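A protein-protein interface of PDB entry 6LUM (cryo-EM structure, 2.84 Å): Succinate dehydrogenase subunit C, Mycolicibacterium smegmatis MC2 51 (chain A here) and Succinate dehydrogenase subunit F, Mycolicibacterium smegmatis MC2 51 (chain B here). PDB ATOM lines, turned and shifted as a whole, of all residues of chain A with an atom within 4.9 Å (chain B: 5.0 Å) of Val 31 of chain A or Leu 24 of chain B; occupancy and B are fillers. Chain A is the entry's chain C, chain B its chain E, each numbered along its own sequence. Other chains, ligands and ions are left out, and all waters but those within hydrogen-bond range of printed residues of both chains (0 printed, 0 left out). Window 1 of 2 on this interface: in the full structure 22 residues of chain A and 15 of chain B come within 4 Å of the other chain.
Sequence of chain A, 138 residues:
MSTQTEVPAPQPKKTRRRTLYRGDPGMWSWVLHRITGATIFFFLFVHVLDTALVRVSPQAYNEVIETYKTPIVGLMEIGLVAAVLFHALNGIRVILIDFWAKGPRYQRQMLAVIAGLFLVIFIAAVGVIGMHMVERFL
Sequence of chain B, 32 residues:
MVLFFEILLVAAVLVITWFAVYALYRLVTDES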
ATOM      1  N   MET A  27      -4.155  12.028   6.600  1.00  0.00           N
ATOM      2  CA  MET A  27      -3.383  10.893   6.123  1.00  0.00           C
ATOM      3  C   MET A  27      -2.185  10.633   7.014  1.00  0.00           C
ATOM      4  O   MET A  27      -1.878   9.483   7.335  1.00  0.00           O
ATOM      5  CB  MET A  27      -2.950  11.149   4.690  1.00  0.00           C
ATOM      6  CG  MET A  27      -2.232  10.024   4.028  1.00  0.00           C
ATOM      7  SD  MET A  27      -1.179  10.690   2.746  1.00  0.00           S
ATOM      8  CE  MET A  27      -0.661   9.189   1.976  1.00  0.00           C
ATOM      9  N   TRP A  28      -1.505  11.689   7.447  1.00  0.00           N
ATOM     10  CA  TRP A  28      -0.374  11.502   8.340  1.00  0.00           C
ATOM     11  C   TRP A  28      -0.826  11.160   9.746  1.00  0.00           C
ATOM     12  O   TRP A  28      -0.147  10.404  10.445  1.00  0.00           O
ATOM     13  CB  TRP A  28       0.495  12.744   8.317  1.00  0.00           C
ATOM     14  CG  TRP A  28       0.859  13.103   6.938  1.00  0.00           C
ATOM     15  CD1 TRP A  28       0.493  14.216   6.262  1.00  0.00           C
ATOM     16  CD2 TRP A  28       1.642  12.324   6.035  1.00  0.00           C
ATOM     17  NE1 TRP A  28       1.007  14.192   4.997  1.00  0.00           N
ATOM     18  CE2 TRP A  28       1.719  13.035   4.834  1.00  0.00           C
ATOM     19  CE3 TRP A  28       2.295  11.097   6.133  1.00  0.00           C
ATOM     20  CZ2 TRP A  28       2.416  12.564   3.740  1.00  0.00           C
ATOM     21  CZ3 TRP A  28       2.985  10.633   5.051  1.00  0.00           C
ATOM     22  CH2 TRP A  28       3.042  11.361   3.869  1.00  0.00           C
ATOM     23  N   SER A  29      -1.974  11.676  10.173  1.00  0.00           N
ATOM     24  CA  SER A  29      -2.566  11.187  11.409  1.00  0.00           C
ATOM     25  C   SER A  29      -2.814   9.693  11.348  1.00  0.00           C
ATOM     26  O   SER A  29      -2.560   8.982  12.316  1.00  0.00           O
ATOM     27  CB  SER A  29      -3.866  11.912  11.689  1.00  0.00           C
ATOM     28  OG  SER A  29      -3.654  13.297  11.649  1.00  0.00           O
ATOM     29  N   TRP A  30      -3.313   9.190  10.223  1.00  0.00           N
ATOM     30  CA  TRP A  30      -3.587   7.762  10.131  1.00  0.00           C
ATOM     31  C   TRP A  30      -2.303   6.949  10.096  1.00  0.00           C
ATOM     32  O   TRP A  30      -2.235   5.865  10.683  1.00  0.00           O
ATOM     33  CB  TRP A  30      -4.438   7.466   8.907  1.00  0.00           C
ATOM     34  CG  TRP A  30      -4.393   6.048   8.496  1.00  0.00           C
ATOM     35  CD1 TRP A  30      -4.942   5.002   9.143  1.00  0.00           C
ATOM     36  CD2 TRP A  30      -3.759   5.513   7.334  1.00  0.00           C
ATOM     37  NE1 TRP A  30      -4.701   3.847   8.463  1.00  0.00           N
ATOM     38  CE2 TRP A  30      -3.969   4.137   7.348  1.00  0.00           C
ATOM     39  CE3 TRP A  30      -3.023   6.067   6.290  1.00  0.00           C
ATOM     40  CZ2 TRP A  30      -3.482   3.310   6.363  1.00  0.00           C
ATOM     41  CZ3 TRP A  30      -2.541   5.246   5.323  1.00  0.00           C
ATOM     42  CH2 TRP A  30      -2.772   3.882   5.361  1.00  0.00           C
ATOM     43  N   VAL A  31      -1.270   7.450   9.425  1.00  0.00           N
ATOM     44  CA  VAL A  31       0.002   6.733   9.405  1.00  0.00           C
ATOM     45  C   VAL A  31       0.581   6.639  10.810  1.00  0.00           C
ATOM     46  O   VAL A  31       1.035   5.574  11.246  1.00  0.00           O
ATOM     47  CB  VAL A  31       0.983   7.411   8.435  1.00  0.00           C
ATOM     48  CG1 VAL A  31       2.298   6.708   8.452  1.00  0.00           C
ATOM     49  CG2 VAL A  31       0.425   7.396   7.050  1.00  0.00           C
ATOM     50  N   LEU A  32       0.558   7.747  11.549  1.00  0.00           N
ATOM     51  CA  LEU A  32       1.058   7.738  12.917  1.00  0.00           C
ATOM     52  C   LEU A  32       0.209   6.868  13.828  1.00  0.00           C
ATOM     53  O   LEU A  32       0.736   6.205  14.720  1.00  0.00           O
ATOM     54  CB  LEU A  32       1.109   9.152  13.455  1.00  0.00           C
ATOM     55  CG  LEU A  32       2.427   9.878  13.340  1.00  0.00           C
ATOM     56  CD1 LEU A  32       2.187  11.339  13.552  1.00  0.00           C
ATOM     57  CD2 LEU A  32       3.333   9.344  14.400  1.00  0.00           C
ATOM     58  N   HIS A  33      -1.106   6.883  13.651  1.00  0.00           N
ATOM     59  CA  HIS A  33      -1.979   6.019  14.430  1.00  0.00           C
ATOM     60  C   HIS A  33      -1.616   4.558  14.227  1.00  0.00           C
ATOM     61  O   HIS A  33      -1.456   3.806  15.190  1.00  0.00           O
ATOM     62  CB  HIS A  33      -3.421   6.278  14.019  1.00  0.00           C
ATOM     63  CG  HIS A  33      -4.430   5.957  15.069  1.00  0.00           C
ATOM     64  ND1 HIS A  33      -5.346   4.943  14.927  1.00  0.00           N
ATOM     65  CD2 HIS A  33      -4.690   6.533  16.260  1.00  0.00           C
ATOM     66  CE1 HIS A  33      -6.118   4.899  15.991  1.00  0.00           C
ATOM     67  NE2 HIS A  33      -5.742   5.854  16.816  1.00  0.00           N
ATOM     68  N   ARG A  34      -1.474   4.142  12.973  1.00  0.00           N
ATOM     69  CA  ARG A  34      -1.125   2.757  12.678  1.00  0.00           C
ATOM     70  C   ARG A  34       0.220   2.382  13.286  1.00  0.00           C
ATOM     71  O   ARG A  34       0.360   1.330  13.924  1.00  0.00           O
ATOM     72  CB  ARG A  34      -1.122   2.559  11.166  1.00  0.00           C
ATOM     73  CG  ARG A  34      -0.524   1.285  10.679  1.00  0.00           C
ATOM     74  CD  ARG A  34      -0.941   1.032   9.261  1.00  0.00           C
ATOM     75  NE  ARG A  34      -2.356   0.716   9.178  1.00  0.00           N
ATOM     76  CZ  ARG A  34      -2.913   0.055   8.177  1.00  0.00           C
ATOM     77  NH1 ARG A  34      -2.171  -0.359   7.174  1.00  0.00           N
ATOM     78  NH2 ARG A  34      -4.207  -0.193   8.183  1.00  0.00           N
ATOM     79  N   ILE A  35       1.217   3.252  13.132  1.00  0.00           N
ATOM     80  CA  ILE A  35       2.561   2.942  13.610  1.00  0.00           C
ATOM     81  C   ILE A  35       2.593   2.844  15.130  1.00  0.00           C
ATOM     82  O   ILE A  35       3.167   1.906  15.694  1.00  0.00           O
ATOM     83  CB  ILE A  35       3.556   3.987  13.089  1.00  0.00           C
ATOM     84  CG1 ILE A  35       3.842   3.749  11.615  1.00  0.00           C
ATOM     85  CG2 ILE A  35       4.827   3.936  13.862  1.00  0.00           C
ATOM     86  CD1 ILE A  35       4.719   4.788  11.009  1.00  0.00           C
ATOM     87  N   PHE B  19       8.716  -2.557  11.397  1.00  0.00           N
ATOM     88  CA  PHE B  19       7.345  -2.285  10.992  1.00  0.00           C
ATOM     89  C   PHE B  19       7.152  -0.819  10.645  1.00  0.00           C
ATOM     90  O   PHE B  19       6.418  -0.497   9.709  1.00  0.00           O
ATOM     91  CB  PHE B  19       6.352  -2.693  12.067  1.00  0.00           C
ATOM     92  CG  PHE B  19       4.944  -2.391  11.691  1.00  0.00           C
ATOM     93  CD1 PHE B  19       4.231  -3.264  10.907  1.00  0.00           C
ATOM     94  CD2 PHE B  19       4.346  -1.212  12.076  1.00  0.00           C
ATOM     95  CE1 PHE B  19       2.952  -2.979  10.539  1.00  0.00           C
ATOM     96  CE2 PHE B  19       3.066  -0.926  11.703  1.00  0.00           C
ATOM     97  CZ  PHE B  19       2.369  -1.808  10.939  1.00  0.00           C
ATOM     98  N   ALA B  20       7.779   0.086  11.391  1.00  0.00           N
ATOM     99  CA  ALA B  20       7.654   1.499  11.047  1.00  0.00           C
ATOM    100  C   ALA B  20       8.153   1.764   9.630  1.00  0.00           C
ATOM    101  O   ALA B  20       7.449   2.371   8.804  1.00  0.00           O
ATOM    102  CB  ALA B  20       8.412   2.354  12.057  1.00  0.00           C
ATOM    103  N   VAL B  21       9.360   1.293   9.314  1.00  0.00           N
ATOM    104  CA  VAL B  21       9.898   1.607   7.994  1.00  0.00           C
ATOM    105  C   VAL B  21       9.137   0.857   6.910  1.00  0.00           C
ATOM    106  O   VAL B  21       9.007   1.349   5.790  1.00  0.00           O
ATOM    107  CB  VAL B  21      11.404   1.316   7.907  1.00  0.00           C
ATOM    108  CG1 VAL B  21      12.200   2.492   8.429  1.00  0.00           C
ATOM    109  CG2 VAL B  21      11.754   0.057   8.614  1.00  0.00           C
ATOM    110  N   TYR B  22       8.591  -0.317   7.218  1.00  0.00           N
ATOM    111  CA  TYR B  22       7.854  -1.065   6.208  1.00  0.00           C
ATOM    112  C   TYR B  22       6.507  -0.427   5.916  1.00  0.00           C
ATOM    113  O   TYR B  22       6.062  -0.415   4.766  1.00  0.00           O
ATOM    114  CB  TYR B  22       7.663  -2.503   6.656  1.00  0.00           C
ATOM    115  CG  TYR B  22       6.973  -3.380   5.647  1.00  0.00           C
ATOM    116  CD1 TYR B  22       7.634  -3.825   4.522  1.00  0.00           C
ATOM    117  CD2 TYR B  22       5.666  -3.782   5.830  1.00  0.00           C
ATOM    118  CE1 TYR B  22       7.013  -4.630   3.610  1.00  0.00           C
ATOM    119  CE2 TYR B  22       5.040  -4.587   4.920  1.00  0.00           C
ATOM    120  CZ  TYR B  22       5.719  -5.007   3.814  1.00  0.00           C
ATOM    121  OH  TYR B  22       5.096  -5.811   2.899  1.00  0.00           O
ATOM    122  N   ALA B  23       5.838   0.104   6.937  1.00  0.00           N
ATOM    123  CA  ALA B  23       4.606   0.836   6.691  1.00  0.00           C
ATOM    124  C   ALA B  23       4.867   2.055   5.824  1.00  0.00           C
ATOM    125  O   ALA B  23       4.138   2.305   4.857  1.00  0.00           O
ATOM    126  CB  ALA B  23       3.961   1.242   8.010  1.00  0.00           C
ATOM    127  N   LEU B  24       5.922   2.812   6.124  1.00  0.00           N
ATOM    128  CA  LEU B  24       6.216   3.969   5.278  1.00  0.00           C
ATOM    129  C   LEU B  24       6.595   3.553   3.859  1.00  0.00           C
ATOM    130  O   LEU B  24       6.228   4.222   2.887  1.00  0.00           O
ATOM    131  CB  LEU B  24       7.317   4.808   5.906  1.00  0.00           C
ATOM    132  CG  LEU B  24       6.833   5.601   7.110  1.00  0.00           C
ATOM    133  CD1 LEU B  24       7.991   6.283   7.779  1.00  0.00           C
ATOM    134  CD2 LEU B  24       5.806   6.608   6.672  1.00  0.00           C
ATOM    135  N   TYR B  25       7.320   2.448   3.719  1.00  0.00           N
ATOM    136  CA  TYR B  25       7.732   1.981   2.403  1.00  0.00           C
ATOM    137  C   TYR B  25       6.532   1.566   1.566  1.00  0.00           C
ATOM    138  O   TYR B  25       6.418   1.944   0.397  1.00  0.00           O
ATOM    139  CB  TYR B  25       8.722   0.831   2.574  1.00  0.00           C
ATOM    140  CG  TYR B  25       8.876  -0.082   1.395  1.00  0.00           C
ATOM    141  CD1 TYR B  25       9.751   0.222   0.374  1.00  0.00           C
ATOM    142  CD2 TYR B  25       8.177  -1.269   1.322  1.00  0.00           C
ATOM    143  CE1 TYR B  25       9.903  -0.616  -0.696  1.00  0.00           C
ATOM    144  CE2 TYR B  25       8.320  -2.111   0.255  1.00  0.00           C
ATOM    145  CZ  TYR B  25       9.182  -1.781  -0.752  1.00  0.00           C
ATOM    146  OH  TYR B  25       9.331  -2.625  -1.822  1.00  0.00           O
ATOM    147  N   ARG B  26       5.621   0.788   2.150  1.00  0.00           N
ATOM    148  CA  ARG B  26       4.411   0.412   1.431  1.00  0.00           C
ATOM    149  C   ARG B  26       3.539   1.620   1.139  1.00  0.00           C
ATOM    150  O   ARG B  26       2.753   1.598   0.190  1.00  0.00           O
ATOM    151  CB  ARG B  26       3.624  -0.617   2.227  1.00  0.00           C
ATOM    152  CG  ARG B  26       4.280  -1.956   2.305  1.00  0.00           C
ATOM    153  CD  ARG B  26       4.310  -2.639   0.967  1.00  0.00           C
ATOM    154  NE  ARG B  26       2.982  -2.792   0.402  1.00  0.00           N
ATOM    155  CZ  ARG B  26       2.285  -3.917   0.427  1.00  0.00           C
ATOM    156  NH1 ARG B  26       2.790  -4.993   0.996  1.00  0.00           N
ATOM    157  NH2 ARG B  26       1.080  -3.959  -0.114  1.00  0.00           N
ATOM    158  N   LEU B  27       3.646   2.675   1.940  1.00  0.00           N
ATOM    159  CA  LEU B  27       2.891   3.881   1.629  1.00  0.00           C
ATOM    160  C   LEU B  27       3.456   4.590   0.408  1.00  0.00           C
ATOM    161  O   LEU B  27       2.700   5.067  -0.439  1.00  0.00           O
ATOM    162  CB  LEU B  27       2.882   4.823   2.828  1.00  0.00           C
ATOM    163  CG  LEU B  27       1.995   6.056   2.741  1.00  0.00           C
ATOM    164  CD1 LEU B  27       0.565   5.674   2.977  1.00  0.00           C
ATOM    165  CD2 LEU B  27       2.443   7.071   3.750  1.00  0.00           C
ATOM    166  N   VAL B  28       4.779   4.679   0.297  1.00  0.00           N
ATOM    167  CA  VAL B  28       5.341   5.493  -0.778  1.00  0.00           C
ATOM    168  C   VAL B  28       5.611   4.746  -2.080  1.00  0.00           C
ATOM    169  O   VAL B  28       5.772   5.395  -3.119  1.00  0.00           O
ATOM    170  CB  VAL B  28       6.638   6.199  -0.354  1.00  0.00           C
ATOM    171  CG1 VAL B  28       6.389   7.055   0.855  1.00  0.00           C
ATOM    172  CG2 VAL B  28       7.726   5.197  -0.098  1.00  0.00           C
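Met 27 of chain A touches Leu 27 of chain B.
CD2 of Leu 27 of chain B touches CZ3 of Trp 28 of chain A, at 3.8 Å.
Leu 27 of chain B touches Trp 30 of chain A (CD1 to CZ3, 3.9 Å).
Val 31 of chain A touches Leu 24 of chain B.
CD2 of Leu 27 of chain B touches CG2 of Val 31 of chain A, 3.9 Å away.
Printed residues of chain B within 4 Å of Trp 28 of chain A: Leu 27 (3.8 Å).
Of chain B, only Leu 24 and Leu 27 come within 4 Å of Val 31 of chain A.
Of chain A, only Val 31 (3.9 Å) comes within 4 Å of Leu 24 of chain B.
Printed residues of chain A within 4 Å of Leu 27 of chain B: Met 27 (3.9 Å), Trp 28 (3.8 Å), Trp 30 (3.9 Å) and Val 31 (3.9 Å).
The nearest residue of chain A that does not touch Leu 24 of chain B is Ile 35 of chain A (4.5 Å).
Of the 10 printed residues of chain B, 2 touch a printed residue of chain A.
Of the 9 printed residues of chain A, 4 touch a printed residue of chain B.
Among the printed residues, no Asp or Glu carboxylate lies within 4 Å of a Lys or Arg side-chain nitrogen of the other chain.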
